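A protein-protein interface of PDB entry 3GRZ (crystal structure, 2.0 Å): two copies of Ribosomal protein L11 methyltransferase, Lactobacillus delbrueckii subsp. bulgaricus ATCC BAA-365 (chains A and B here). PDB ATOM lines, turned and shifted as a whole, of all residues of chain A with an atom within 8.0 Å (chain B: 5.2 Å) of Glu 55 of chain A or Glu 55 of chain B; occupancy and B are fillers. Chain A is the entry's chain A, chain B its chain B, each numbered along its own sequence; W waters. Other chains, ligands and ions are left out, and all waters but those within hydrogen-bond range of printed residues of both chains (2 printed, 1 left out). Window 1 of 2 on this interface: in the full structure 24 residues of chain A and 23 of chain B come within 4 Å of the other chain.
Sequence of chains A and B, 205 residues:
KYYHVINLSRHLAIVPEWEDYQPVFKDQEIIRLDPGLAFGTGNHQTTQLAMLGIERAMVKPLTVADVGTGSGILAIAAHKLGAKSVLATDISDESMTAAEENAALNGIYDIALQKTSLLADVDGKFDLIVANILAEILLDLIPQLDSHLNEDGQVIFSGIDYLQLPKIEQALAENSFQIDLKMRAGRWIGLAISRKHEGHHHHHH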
ATOM      1  N   ASN A   7     -34.050   1.158  23.206  1.00  0.00           N
ATOM      2  CA  ASN A   7     -32.600   1.080  23.206  1.00  0.00           C
ATOM      3  C   ASN A   7     -32.037   2.456  23.442  1.00  0.00           C
ATOM      4  O   ASN A   7     -31.815   3.206  22.484  1.00  0.00           O
ATOM      5  CB  ASN A   7     -32.142   0.590  21.839  1.00  0.00           C
ATOM      6  CG  ASN A   7     -31.223  -0.585  21.921  1.00  0.00           C
ATOM      7  OD1 ASN A   7     -30.615  -0.849  22.957  1.00  0.00           O
ATOM      8  ND2 ASN A   7     -31.109  -1.309  20.819  1.00  0.00           N
ATOM      9  N   LEU A   8     -31.821   2.789  24.713  1.00  0.00           N
ATOM     10  CA  LEU A   8     -31.440   4.143  25.112  1.00  0.00           C
ATOM     11  C   LEU A   8     -29.991   4.504  24.795  1.00  0.00           C
ATOM     12  O   LEU A   8     -29.716   5.576  24.244  1.00  0.00           O
ATOM     13  CB  LEU A   8     -31.694   4.360  26.603  1.00  0.00           C
ATOM     14  CG  LEU A   8     -33.146   4.492  27.074  1.00  0.00           C
ATOM     15  CD1 LEU A   8     -33.171   4.592  28.576  1.00  0.00           C
ATOM     16  CD2 LEU A   8     -33.843   5.698  26.464  1.00  0.00           C
ATOM     17  N   SER A   9     -29.076   3.606  25.158  1.00  0.00           N
ATOM     18  CA  SER A   9     -27.647   3.861  25.050  1.00  0.00           C
ATOM     19  C   SER A   9     -26.863   2.561  25.088  1.00  0.00           C
ATOM     20  O   SER A   9     -27.433   1.455  25.199  1.00  0.00           O
ATOM     21  CB  SER A   9     -27.176   4.774  26.196  1.00  0.00           C
ATOM     22  OG  SER A   9     -27.219   4.095  27.448  1.00  0.00           O
ATOM     23  N   ARG A  10     -25.543   2.706  25.023  1.00  0.00           N
ATOM     24  CA  ARG A  10     -24.624   1.591  25.149  1.00  0.00           C
ATOM     25  C   ARG A  10     -24.894   0.773  26.410  1.00  0.00           C
ATOM     26  O   ARG A  10     -24.831  -0.455  26.397  1.00  0.00           O
ATOM     27  CB  ARG A  10     -23.179   2.118  25.141  1.00  0.00           C
ATOM     28  CG  ARG A  10     -22.116   1.095  25.486  1.00  0.00           C
ATOM     29  CD  ARG A  10     -22.084  -0.061  24.506  1.00  0.00           C
ATOM     30  NE  ARG A  10     -21.101  -1.088  24.838  1.00  0.00           N
ATOM     31  CZ  ARG A  10     -21.252  -2.030  25.765  1.00  0.00           C
ATOM     32  NH1 ARG A  10     -22.361  -2.103  26.508  1.00  0.00           N
ATOM     33  NH2 ARG A  10     -20.275  -2.907  25.953  1.00  0.00           N
ATOM     34  N   HIS A  11     -25.204   1.452  27.500  1.00  0.00           N
ATOM     35  CA  HIS A  11     -25.301   0.758  28.778  1.00  0.00           C
ATOM     36  C   HIS A  11     -26.708   0.538  29.301  1.00  0.00           C
ATOM     37  O   HIS A  11     -26.873  -0.018  30.375  1.00  0.00           O
ATOM     38  CB  HIS A  11     -24.440   1.466  29.811  1.00  0.00           C
ATOM     39  CG  HIS A  11     -22.988   1.479  29.446  1.00  0.00           C
ATOM     40  ND1 HIS A  11     -22.397   2.550  28.820  1.00  0.00           N
ATOM     41  CD2 HIS A  11     -22.023   0.538  29.578  1.00  0.00           C
ATOM     42  CE1 HIS A  11     -21.121   2.283  28.608  1.00  0.00           C
ATOM     43  NE2 HIS A  11     -20.870   1.066  29.054  1.00  0.00           N
ATOM     44  N   LEU A  12     -27.720   0.923  28.531  1.00  0.00           N
ATOM     45  CA  LEU A  12     -29.081   0.811  29.029  1.00  0.00           C
ATOM     46  C   LEU A  12     -30.137   0.589  27.969  1.00  0.00           C
ATOM     47  O   LEU A  12     -30.217   1.328  26.980  1.00  0.00           O
ATOM     48  CB  LEU A  12     -29.450   2.067  29.827  1.00  0.00           C
ATOM     49  CG  LEU A  12     -30.443   1.868  30.968  1.00  0.00           C
ATOM     50  CD1 LEU A  12     -29.743   1.284  32.193  1.00  0.00           C
ATOM     51  CD2 LEU A  12     -31.077   3.202  31.299  1.00  0.00           C
ATOM     52  N   GLN A  28     -24.924  -4.465  28.566  1.00  0.00           N
ATOM     53  CA  GLN A  28     -25.960  -3.431  28.482  1.00  0.00           C
ATOM     54  C   GLN A  28     -27.033  -3.770  29.500  1.00  0.00           C
ATOM     55  O   GLN A  28     -27.701  -4.792  29.372  1.00  0.00           O
ATOM     56  CB  GLN A  28     -26.578  -3.350  27.088  1.00  0.00           C
ATOM     57  CG  GLN A  28     -27.640  -2.243  26.967  1.00  0.00           C
ATOM     58  CD  GLN A  28     -28.353  -2.264  25.634  1.00  0.00           C
ATOM     59  OE1 GLN A  28     -28.741  -3.327  25.142  1.00  0.00           O
ATOM     60  NE2 GLN A  28     -28.531  -1.092  25.038  1.00  0.00           N
ATOM     61  N   GLN A  48     -35.032   9.748  27.426  1.00  0.00           N
ATOM     62  CA  GLN A  48     -33.674   9.657  26.910  1.00  0.00           C
ATOM     63  C   GLN A  48     -32.817  10.876  27.270  1.00  0.00           C
ATOM     64  O   GLN A  48     -31.649  10.719  27.616  1.00  0.00           O
ATOM     65  CB  GLN A  48     -33.621   9.392  25.402  1.00  0.00           C
ATOM     66  CG  GLN A  48     -32.224   8.902  24.961  1.00  0.00           C
ATOM     67  CD  GLN A  48     -32.005   8.877  23.456  1.00  0.00           C
ATOM     68  OE1 GLN A  48     -32.317   9.837  22.749  1.00  0.00           O
ATOM     69  NE2 GLN A  48     -31.436   7.775  22.964  1.00  0.00           N
ATOM     70  N   LEU A  49     -33.393  12.076  27.205  1.00  0.00           N
ATOM     71  CA  LEU A  49     -32.643  13.286  27.591  1.00  0.00           C
ATOM     72  C   LEU A  49     -32.254  13.255  29.077  1.00  0.00           C
ATOM     73  O   LEU A  49     -31.110  13.555  29.418  1.00  0.00           O
ATOM     74  CB  LEU A  49     -33.415  14.572  27.256  1.00  0.00           C
ATOM     75  CG  LEU A  49     -33.846  14.799  25.793  1.00  0.00           C
ATOM     76  CD1 LEU A  49     -34.752  16.026  25.615  1.00  0.00           C
ATOM     77  CD2 LEU A  49     -32.649  14.879  24.854  1.00  0.00           C
ATOM     78  N   ALA A  50     -33.199  12.882  29.939  1.00  0.00           N
ATOM     79  CA  ALA A  50     -32.956  12.789  31.391  1.00  0.00           C
ATOM     80  C   ALA A  50     -31.874  11.743  31.700  1.00  0.00           C
ATOM     81  O   ALA A  50     -30.996  11.980  32.532  1.00  0.00           O
ATOM     82  CB  ALA A  50     -34.258  12.456  32.145  1.00  0.00           C
ATOM     83  N   MET A  51     -31.943  10.611  31.001  1.00  0.00           N
ATOM     84  CA  MET A  51     -30.923   9.567  31.069  1.00  0.00           C
ATOM     85  C   MET A  51     -29.513  10.009  30.676  1.00  0.00           C
ATOM     86  O   MET A  51     -28.542   9.652  31.348  1.00  0.00           O
ATOM     87  CB  MET A  51     -31.339   8.340  30.244  1.00  0.00           C
ATOM     88  CG  MET A  51     -32.267   7.391  30.976  1.00  0.00           C
ATOM     89  SD  MET A  51     -31.853   7.107  32.716  1.00  0.00           S
ATOM     90  CE  MET A  51     -30.138   6.535  32.609  1.00  0.00           C
ATOM     91  N   LEU A  52     -29.399  10.773  29.591  1.00  0.00           N
ATOM     92  CA  LEU A  52     -28.116  11.355  29.209  1.00  0.00           C
ATOM     93  C   LEU A  52     -27.538  12.269  30.283  1.00  0.00           C
ATOM     94  O   LEU A  52     -26.320  12.255  30.525  1.00  0.00           O
ATOM     95  CB  LEU A  52     -28.229  12.112  27.887  1.00  0.00           C
ATOM     96  CG  LEU A  52     -28.317  11.249  26.619  1.00  0.00           C
ATOM     97  CD1 LEU A  52     -28.286  12.151  25.398  1.00  0.00           C
ATOM     98  CD2 LEU A  52     -27.213  10.186  26.538  1.00  0.00           C
ATOM     99  N   GLY A  53     -28.413  13.058  30.909  1.00  0.00           N
ATOM    100  CA  GLY A  53     -28.044  13.907  32.031  1.00  0.00           C
ATOM    101  C   GLY A  53     -27.492  13.094  33.187  1.00  0.00           C
ATOM    102  O   GLY A  53     -26.468  13.464  33.768  1.00  0.00           O
ATOM    103  N   ILE A  54     -28.172  11.992  33.506  1.00  0.00           N
ATOM    104  CA  ILE A  54     -27.783  11.100  34.616  1.00  0.00           C
ATOM    105  C   ILE A  54     -26.458  10.400  34.308  1.00  0.00           C
ATOM    106  O   ILE A  54     -25.613  10.257  35.191  1.00  0.00           O
ATOM    107  CB  ILE A  54     -28.885  10.035  34.936  1.00  0.00           C
ATOM    108  CG1 ILE A  54     -30.193  10.705  35.383  1.00  0.00           C
ATOM    109  CG2 ILE A  54     -28.413   9.056  36.053  1.00  0.00           C
ATOM    110  CD1 ILE A  54     -31.361   9.711  35.608  1.00  0.00           C
ATOM    111  N   GLU A  55     -26.298   9.966  33.057  1.00  0.00           N
ATOM    112  CA  GLU A  55     -25.068   9.302  32.577  1.00  0.00           C
ATOM    113  C   GLU A  55     -23.860  10.231  32.723  1.00  0.00           C
ATOM    114  O   GLU A  55     -22.804   9.820  33.204  1.00  0.00           O
ATOM    115  CB  GLU A  55     -25.249   8.845  31.111  1.00  0.00           C
ATOM    116  CG  GLU A  55     -23.984   8.370  30.374  1.00  0.00           C
ATOM    117  CD  GLU A  55     -23.448   7.024  30.853  1.00  0.00           C
ATOM    118  OE1 GLU A  55     -24.220   6.214  31.423  1.00  0.00           O
ATOM    119  OE2 GLU A  55     -22.237   6.779  30.651  1.00  0.00           O
ATOM    120  N   ARG A  56     -24.042  11.485  32.329  1.00  0.00           N
ATOM    121  CA  ARG A  56     -23.037  12.525  32.492  1.00  0.00           C
ATOM    122  C   ARG A  56     -22.710  12.797  33.970  1.00  0.00           C
ATOM    123  O   ARG A  56     -21.540  12.847  34.341  1.00  0.00           O
ATOM    124  CB  ARG A  56     -23.511  13.794  31.797  1.00  0.00           C
ATOM    125  CG  ARG A  56     -22.582  14.994  31.876  1.00  0.00           C
ATOM    126  CD  ARG A  56     -23.304  16.205  31.332  1.00  0.00           C
ATOM    127  NE  ARG A  56     -22.516  17.428  31.386  1.00  0.00           N
ATOM    128  CZ  ARG A  56     -22.543  18.304  32.385  1.00  0.00           C
ATOM    129  NH1 ARG A  56     -21.787  19.383  32.321  1.00  0.00           N
ATOM    130  NH2 ARG A  56     -23.315  18.108  33.446  1.00  0.00           N
ATOM    131  N   ALA A  57     -23.747  12.924  34.800  1.00  0.00           N
ATOM    132  CA  ALA A  57     -23.605  13.333  36.200  1.00  0.00           C
ATOM    133  C   ALA A  57     -23.040  12.267  37.146  1.00  0.00           C
ATOM    134  O   ALA A  57     -22.335  12.603  38.092  1.00  0.00           O
ATOM    135  CB  ALA A  57     -24.949  13.832  36.734  1.00  0.00           C
ATOM    136  N   MET A  58     -23.374  10.995  36.924  1.00  0.00           N
ATOM    137  CA  MET A  58     -23.023   9.939  37.879  1.00  0.00           C
ATOM    138  C   MET A  58     -21.551   9.470  37.772  1.00  0.00           C
ATOM    139  O   MET A  58     -21.284   8.333  37.414  1.00  0.00           O
ATOM    140  CB  MET A  58     -23.984   8.740  37.763  1.00  0.00           C
ATOM    141  CG  MET A  58     -24.037   7.820  39.033  1.00  0.00           C
ATOM    142  SD  MET A  58     -24.923   8.464  40.477  1.00  0.00           S
ATOM    143  CE  MET A  58     -26.596   8.365  39.874  1.00  0.00           C
ATOM    144  N   VAL A  59     -20.601  10.327  38.131  1.00  0.00           N
ATOM    145  CA  VAL A  59     -19.177   9.943  38.057  1.00  0.00           C
ATOM    146  C   VAL A  59     -18.681   9.231  39.327  1.00  0.00           C
ATOM    147  O   VAL A  59     -17.586   8.657  39.346  1.00  0.00           O
ATOM    148  CB  VAL A  59     -18.271  11.143  37.701  1.00  0.00           C
ATOM    149  CG1 VAL A  59     -18.723  11.758  36.385  1.00  0.00           C
ATOM    150  CG2 VAL A  59     -18.266  12.182  38.836  1.00  0.00           C
ATOM    151  N   LYS A  60     -19.509   9.272  40.371  1.00  0.00           N
ATOM    152  CA  LYS A  60     -19.267   8.594  41.641  1.00  0.00           C
ATOM    153  C   LYS A  60     -20.656   8.303  42.217  1.00  0.00           C
ATOM    154  O   LYS A  60     -21.640   8.817  41.672  1.00  0.00           O
ATOM    155  CB  LYS A  60     -18.414   9.474  42.570  1.00  0.00           C
ATOM    156  CG  LYS A  60     -19.060  10.769  43.014  1.00  0.00           C
ATOM    157  CD  LYS A  60     -18.196  11.462  44.050  1.00  0.00           C
ATOM    158  CE  LYS A  60     -18.908  12.655  44.653  1.00  0.00           C
ATOM    159  NZ  LYS A  60     -18.025  13.386  45.606  1.00  0.00           N
ATOM    160  N   ALA A  77     -33.081   3.557  37.059  1.00  0.00           N
ATOM    161  CA  ALA A  77     -31.865   3.770  36.267  1.00  0.00           C
ATOM    162  C   ALA A  77     -30.711   4.359  37.082  1.00  0.00           C
ATOM    163  O   ALA A  77     -29.571   3.901  36.961  1.00  0.00           O
ATOM    164  CB  ALA A  77     -32.167   4.647  35.090  1.00  0.00           C
ATOM    165  N   ALA A  78     -31.012   5.360  37.908  1.00  0.00           N
ATOM    166  CA  ALA A  78     -30.017   5.969  38.799  1.00  0.00           C
ATOM    167  C   ALA A  78     -29.442   4.928  39.761  1.00  0.00           C
ATOM    168  O   ALA A  78     -28.227   4.890  39.993  1.00  0.00           O
ATOM    169  CB  ALA A  78     -30.629   7.140  39.572  1.00  0.00           C
ATOM    170  N   LEU A  81     -27.145   2.646  37.858  1.00  0.00           N
ATOM    171  CA  LEU A  81     -25.901   3.353  37.532  1.00  0.00           C
ATOM    172  C   LEU A  81     -25.049   3.638  38.768  1.00  0.00           C
ATOM    173  O   LEU A  81     -23.991   4.262  38.677  1.00  0.00           O
ATOM    174  CB  LEU A  81     -26.196   4.637  36.758  1.00  0.00           C
ATOM    175  CG  LEU A  81     -26.575   4.451  35.297  1.00  0.00           C
ATOM    176  CD1 LEU A  81     -26.875   5.800  34.658  1.00  0.00           C
ATOM    177  CD2 LEU A  81     -25.454   3.757  34.548  1.00  0.00           C
ATOM    178  N   LEU A 128     -27.964  14.913  43.666  1.00  0.00           N
ATOM    179  CA  LEU A 128     -28.570  14.950  42.332  1.00  0.00           C
ATOM    180  C   LEU A 128     -30.095  14.991  42.409  1.00  0.00           C
ATOM    181  O   LEU A 128     -30.715  14.114  42.998  1.00  0.00           O
ATOM    182  CB  LEU A 128     -28.106  13.747  41.498  1.00  0.00           C
ATOM    183  CG  LEU A 128     -28.532  13.718  40.020  1.00  0.00           C
ATOM    184  CD1 LEU A 128     -27.928  14.887  39.277  1.00  0.00           C
ATOM    185  CD2 LEU A 128     -28.124  12.392  39.371  1.00  0.00           C
ATOM    186  N   ILE A 156     -31.053  17.709  37.108  1.00  0.00           N
ATOM    187  CA  ILE A 156     -31.404  17.329  35.746  1.00  0.00           C
ATOM    188  C   ILE A 156     -32.908  17.520  35.525  1.00  0.00           C
ATOM    189  O   ILE A 156     -33.712  16.932  36.243  1.00  0.00           O
ATOM    190  CB  ILE A 156     -31.009  15.869  35.442  1.00  0.00           C
ATOM    191  CG1 ILE A 156     -29.496  15.677  35.605  1.00  0.00           C
ATOM    192  CG2 ILE A 156     -31.424  15.476  34.013  1.00  0.00           C
ATOM    193  CD1 ILE A 156     -29.142  14.272  35.944  1.00  0.00           C
ATOM    194  N   SER B   9     -18.150  10.980  32.008  1.00  0.00           N
ATOM    195  CA  SER B   9     -19.440  10.370  32.307  1.00  0.00           C
ATOM    196  C   SER B   9     -19.268   9.275  33.346  1.00  0.00           C
ATOM    197  O   SER B   9     -18.156   9.045  33.836  1.00  0.00           O
ATOM    198  CB  SER B   9     -20.070   9.807  31.027  1.00  0.00           C
ATOM    199  OG  SER B   9     -19.411   8.638  30.572  1.00  0.00           O
ATOM    200  N   ARG B  10     -20.373   8.607  33.667  1.00  0.00           N
ATOM    201  CA  ARG B  10     -20.395   7.401  34.478  1.00  0.00           C
ATOM    202  C   ARG B  10     -19.450   6.306  33.957  1.00  0.00           C
ATOM    203  O   ARG B  10     -18.878   5.533  34.740  1.00  0.00           O
ATOM    204  CB  ARG B  10     -21.847   6.880  34.560  1.00  0.00           C
ATOM    205  CG  ARG B  10     -22.053   5.461  35.117  1.00  0.00           C
ATOM    206  CD  ARG B  10     -21.604   5.325  36.565  1.00  0.00           C
ATOM    207  NE  ARG B  10     -21.721   3.968  37.110  1.00  0.00           N
ATOM    208  CZ  ARG B  10     -20.883   2.964  36.844  1.00  0.00           C
ATOM    209  NH1 ARG B  10     -19.844   3.136  36.034  1.00  0.00           N
ATOM    210  NH2 ARG B  10     -21.083   1.777  37.396  1.00  0.00           N
ATOM    211  N   HIS B  11     -19.290   6.243  32.643  1.00  0.00           N
ATOM    212  CA  HIS B  11     -18.529   5.159  32.049  1.00  0.00           C
ATOM    213  C   HIS B  11     -17.213   5.584  31.402  1.00  0.00           C
ATOM    214  O   HIS B  11     -16.540   4.752  30.810  1.00  0.00           O
ATOM    215  CB  HIS B  11     -19.401   4.398  31.049  1.00  0.00           C
ATOM    216  CG  HIS B  11     -20.550   3.681  31.686  1.00  0.00           C
ATOM    217  ND1 HIS B  11     -21.845   4.147  31.619  1.00  0.00           N
ATOM    218  CD2 HIS B  11     -20.593   2.545  32.424  1.00  0.00           C
ATOM    219  CE1 HIS B  11     -22.640   3.320  32.274  1.00  0.00           C
ATOM    220  NE2 HIS B  11     -21.906   2.341  32.772  1.00  0.00           N
ATOM    221  N   ALA B  50     -19.197  15.019  22.142  1.00  0.00           N
ATOM    222  CA  ALA B  50     -18.959  13.917  21.200  1.00  0.00           C
ATOM    223  C   ALA B  50     -19.128  12.551  21.883  1.00  0.00           C
ATOM    224  O   ALA B  50     -19.826  11.680  21.361  1.00  0.00           O
ATOM    225  CB  ALA B  50     -17.577  14.047  20.555  1.00  0.00           C
ATOM    226  N   MET B  51     -18.543  12.394  23.074  1.00  0.00           N
ATOM    227  CA  MET B  51     -18.678  11.155  23.851  1.00  0.00           C
ATOM    228  C   MET B  51     -20.103  10.773  24.223  1.00  0.00           C
ATOM    229  O   MET B  51     -20.449   9.587  24.187  1.00  0.00           O
ATOM    230  CB  MET B  51     -17.838  11.197  25.146  1.00  0.00           C
ATOM    231  CG  MET B  51     -16.348  11.075  24.935  1.00  0.00           C
ATOM    232  SD  MET B  51     -15.868   9.565  24.080  1.00  0.00           S
ATOM    233  CE  MET B  51     -16.989   8.345  24.816  1.00  0.00           C
ATOM    234  N   LEU B  52     -20.914  11.764  24.605  1.00  0.00           N
ATOM    235  CA  LEU B  52     -22.337  11.528  24.911  1.00  0.00           C
ATOM    236  C   LEU B  52     -23.088  11.041  23.676  1.00  0.00           C
ATOM    237  O   LEU B  52     -23.945  10.164  23.775  1.00  0.00           O
ATOM    238  CB  LEU B  52     -23.007  12.783  25.479  1.00  0.00           C
ATOM    239  CG  LEU B  52     -22.549  13.238  26.867  1.00  0.00           C
ATOM    240  CD1 LEU B  52     -23.215  14.566  27.279  1.00  0.00           C
ATOM    241  CD2 LEU B  52     -22.780  12.150  27.915  1.00  0.00           C
ATOM    242  N   GLY B  53     -22.750  11.605  22.520  1.00  0.00           N
ATOM    243  CA  GLY B  53     -23.293  11.131  21.247  1.00  0.00           C
ATOM    244  C   GLY B  53     -22.911   9.693  20.930  1.00  0.00           C
ATOM    245  O   GLY B  53     -23.731   8.935  20.397  1.00  0.00           O
ATOM    246  N   ILE B  54     -21.661   9.321  21.228  1.00  0.00           N
ATOM    247  CA  ILE B  54     -21.184   7.956  20.976  1.00  0.00           C
ATOM    248  C   ILE B  54     -21.874   6.984  21.932  1.00  0.00           C
ATOM    249  O   ILE B  54     -22.327   5.909  21.522  1.00  0.00           O
ATOM    250  CB  ILE B  54     -19.642   7.828  21.089  1.00  0.00           C
ATOM    251  CG1 ILE B  54     -18.945   8.707  20.057  1.00  0.00           C
ATOM    252  CG2 ILE B  54     -19.187   6.366  20.898  1.00  0.00           C
ATOM    253  CD1 ILE B  54     -17.425   8.833  20.280  1.00  0.00           C
ATOM    254  N   GLU B  55     -21.992   7.389  23.193  1.00  0.00           N
ATOM    255  CA  GLU B  55     -22.681   6.594  24.210  1.00  0.00           C
ATOM    256  C   GLU B  55     -24.146   6.341  23.805  1.00  0.00           C
ATOM    257  O   GLU B  55     -24.665   5.243  23.990  1.00  0.00           O
ATOM    258  CB  GLU B  55     -22.590   7.301  25.577  1.00  0.00           C
ATOM    259  CG  GLU B  55     -23.471   6.732  26.699  1.00  0.00           C
ATOM    260  CD  GLU B  55     -22.934   5.439  27.297  1.00  0.00           C
ATOM    261  OE1 GLU B  55     -21.735   5.138  27.112  1.00  0.00           O
ATOM    262  OE2 GLU B  55     -23.713   4.714  27.958  1.00  0.00           O
ATOM    263  N   ARG B  56     -24.777   7.354  23.215  1.00  0.00           N
ATOM    264  CA  ARG B  56     -26.147   7.252  22.748  1.00  0.00           C
ATOM    265  C   ARG B  56     -26.242   6.320  21.549  1.00  0.00           C
ATOM    266  O   ARG B  56     -27.135   5.468  21.496  1.00  0.00           O
ATOM    267  CB  ARG B  56     -26.686   8.646  22.420  1.00  0.00           C
ATOM    268  CG  ARG B  56     -28.062   8.695  21.783  1.00  0.00           C
ATOM    269  CD  ARG B  56     -28.388  10.128  21.377  1.00  0.00           C
ATOM    270  NE  ARG B  56     -29.609  10.231  20.593  1.00  0.00           N
ATOM    271  CZ  ARG B  56     -29.675  10.056  19.275  1.00  0.00           C
ATOM    272  NH1 ARG B  56     -30.838  10.161  18.644  1.00  0.00           N
ATOM    273  NH2 ARG B  56     -28.588   9.759  18.588  1.00  0.00           N
ATOM    274  N   ALA B  57     -25.320   6.479  20.596  1.00  0.00           N
ATOM    275  CA  ALA B  57     -25.383   5.745  19.328  1.00  0.00           C
ATOM    276  C   ALA B  57     -24.987   4.272  19.439  1.00  0.00           C
ATOM    277  O   ALA B  57     -25.497   3.448  18.691  1.00  0.00           O
ATOM    278  CB  ALA B  57     -24.536   6.441  18.243  1.00  0.00           C
ATOM    279  N   MET B  58     -24.084   3.933  20.364  1.00  0.00           N
ATOM    280  CA  MET B  58     -23.497   2.587  20.373  1.00  0.00           C
ATOM    281  C   MET B  58     -24.369   1.577  21.101  1.00  0.00           C
ATOM    282  O   MET B  58     -23.988   1.059  22.145  1.00  0.00           O
ATOM    283  CB  MET B  58     -22.040   2.586  20.913  1.00  0.00           C
ATOM    284  CG  MET B  58     -21.185   1.363  20.471  1.00  0.00           C
ATOM    285  SD  MET B  58     -20.532   1.369  18.765  1.00  0.00           S
ATOM    286  CE  MET B  58     -19.196   2.564  18.954  1.00  0.00           C
ATOM    287  N   LEU B  81     -16.009   1.153  23.814  1.00  0.00           N
ATOM    288  CA  LEU B  81     -17.473   1.049  23.860  1.00  0.00           C
ATOM    289  C   LEU B  81     -18.047  -0.024  22.940  1.00  0.00           C
ATOM    290  O   LEU B  81     -19.264  -0.153  22.826  1.00  0.00           O
ATOM    291  CB  LEU B  81     -18.129   2.406  23.584  1.00  0.00           C
ATOM    292  CG  LEU B  81     -17.965   3.423  24.719  1.00  0.00           C
ATOM    293  CD1 LEU B  81     -18.471   4.786  24.302  1.00  0.00           C
ATOM    294  CD2 LEU B  81     -18.645   2.972  26.003  1.00  0.00           C
HETATM  295  O   HOH W   1     -23.226   0.883  38.881  1.00  0.00           O
HETATM  296  O   HOH W   2     -25.933   5.224  29.502  1.00  0.00           O
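ND1 of His 11 of chain B sits at hydrogen-bond distance from OE2 of Glu 55 of chain A (2.8 Å). The guanidinium group of Arg 10 of chain A lies within hydrogen-bond range of the backbone carbonyl oxygen of Leu 81 of chain B (2.9 Å). N of Arg 10 of chain A lies within hydrogen-bond range of O of Glu 55 of chain B (2.9 Å). The side-chain amide oxygen (OE1) of Gln 48 of chain A is in hydrogen-bond range of the guanidinium group (NE) of Arg 56 of chain B (3.5 Å). The side-chain carboxylate (OE2) of Glu 55 of chain A is in hydrogen-bond range of the side-chain hydroxyl (OG) of Ser 9 of chain B (3.4 Å). O of Leu 81 of chain A is in hydrogen-bond range of NE of Arg 10 of chain B (2.8 Å). The backbone NH (N) of Arg 10 of chain B sits at hydrogen-bond distance from the backbone carbonyl oxygen (O) of Glu 55 of chain A (2.8 Å). ND1 of His 11 of chain A is in hydrogen-bond range of ND1 of His 11 of chain B, at 3.3 Å. OE2 of Glu 55 of chain B lies within hydrogen-bond range of ND1 of His 11 of chain A, at 2.7 Å.
N of Leu 12 of chain A lies within hydrogen-bond range of OG of Ser 9 of chain A, 3.4 Å away. NE2 of Gln 48 of chain A is in hydrogen-bond range of O of Leu 8 of chain A. The side-chain hydroxyl of Ser 9 of chain A sits close to the backbone NH of His 11 of chain A, at 3.3 Å.
O of Leu 8 of chain A touches O of Arg 56 of chain B, at 3.8 Å. Arg 56 of chain B touches Ser 9 of chain A. Arg 10 of chain A touches Met 58 of chain B (CA to O, 3.1 Å). Leu 81 of chain B touches His 11 of chain A (CD2 to CE1, 3.7 Å). OE2 of Glu 55 of chain A touches CD of Glu 55 of chain B, 3.7 Å away. CA of Ser 9 of chain B touches O of Arg 56 of chain A, 3.8 Å away. Leu 81 of chain A touches His 11 of chain B.
Printed residues of chain B within 4 Å of Gln 48 of chain A: Arg 56. Glu 55 of chain A touches just these residues of chain B: Ser 9, Arg 10, His 11 and Glu 55. Of the printed residues of chain A, Ser 9 of chain B touches Glu 55, Arg 56 and Val 59. Of the printed residues of chain A, Glu 55 of chain B touches Ser 9, Arg 10, His 11 and Glu 55. Of the printed residues of chain A, Leu 81 of chain B touches Arg 10 (2.9 Å) and His 11 (3.7 Å). The nearest residue of chain B that does not touch Glu 55 of chain A is Leu 52 of chain B (4.7 Å). The nearest printed residue of chain A that does not touch Glu 55 of chain B is Leu 8 of chain A (5.1 Å).
Of the 13 printed residues of chain B, 7 touch a printed residue of chain A. Hydrophobic or aromatic side chains of chain B that line the printed part of chain A: His 11 and Leu 81. Along chain B the printed residues that touch a printed residue of chain A span positions 9 to 81. Hydrophobic or aromatic side chains of chain A within 4 Å of the printed part of chain B: His 11, Val 59 and Leu 81. Among the printed residues, 19 pairs touch across the chains.
Arg 10 of chain A touches Met 58 of chain B, and with the chains exchanged Met 58 of chain A touches Arg 10 of chain B. His 11 of chain A touches Leu 81 of chain B, and with the chains exchanged Leu 81 of chain A touches His 11 of chain B. Of the 19 pairs that touch across the chains among the printed residues, 16 have their exchanged pair printed and touching as well.
Water W2 lies within hydrogen-bond range of OG of Ser 9 of chain A (2.7 Å), OE2 of Glu 55 of chain B (2.8 Å) and OE1 of Glu 55 of chain A (2.8 Å). Water W1 lies within hydrogen-bond range of the guanidinium group of Arg 10 of chain B and the backbone carbonyl oxygen of Leu 81 of chain A.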
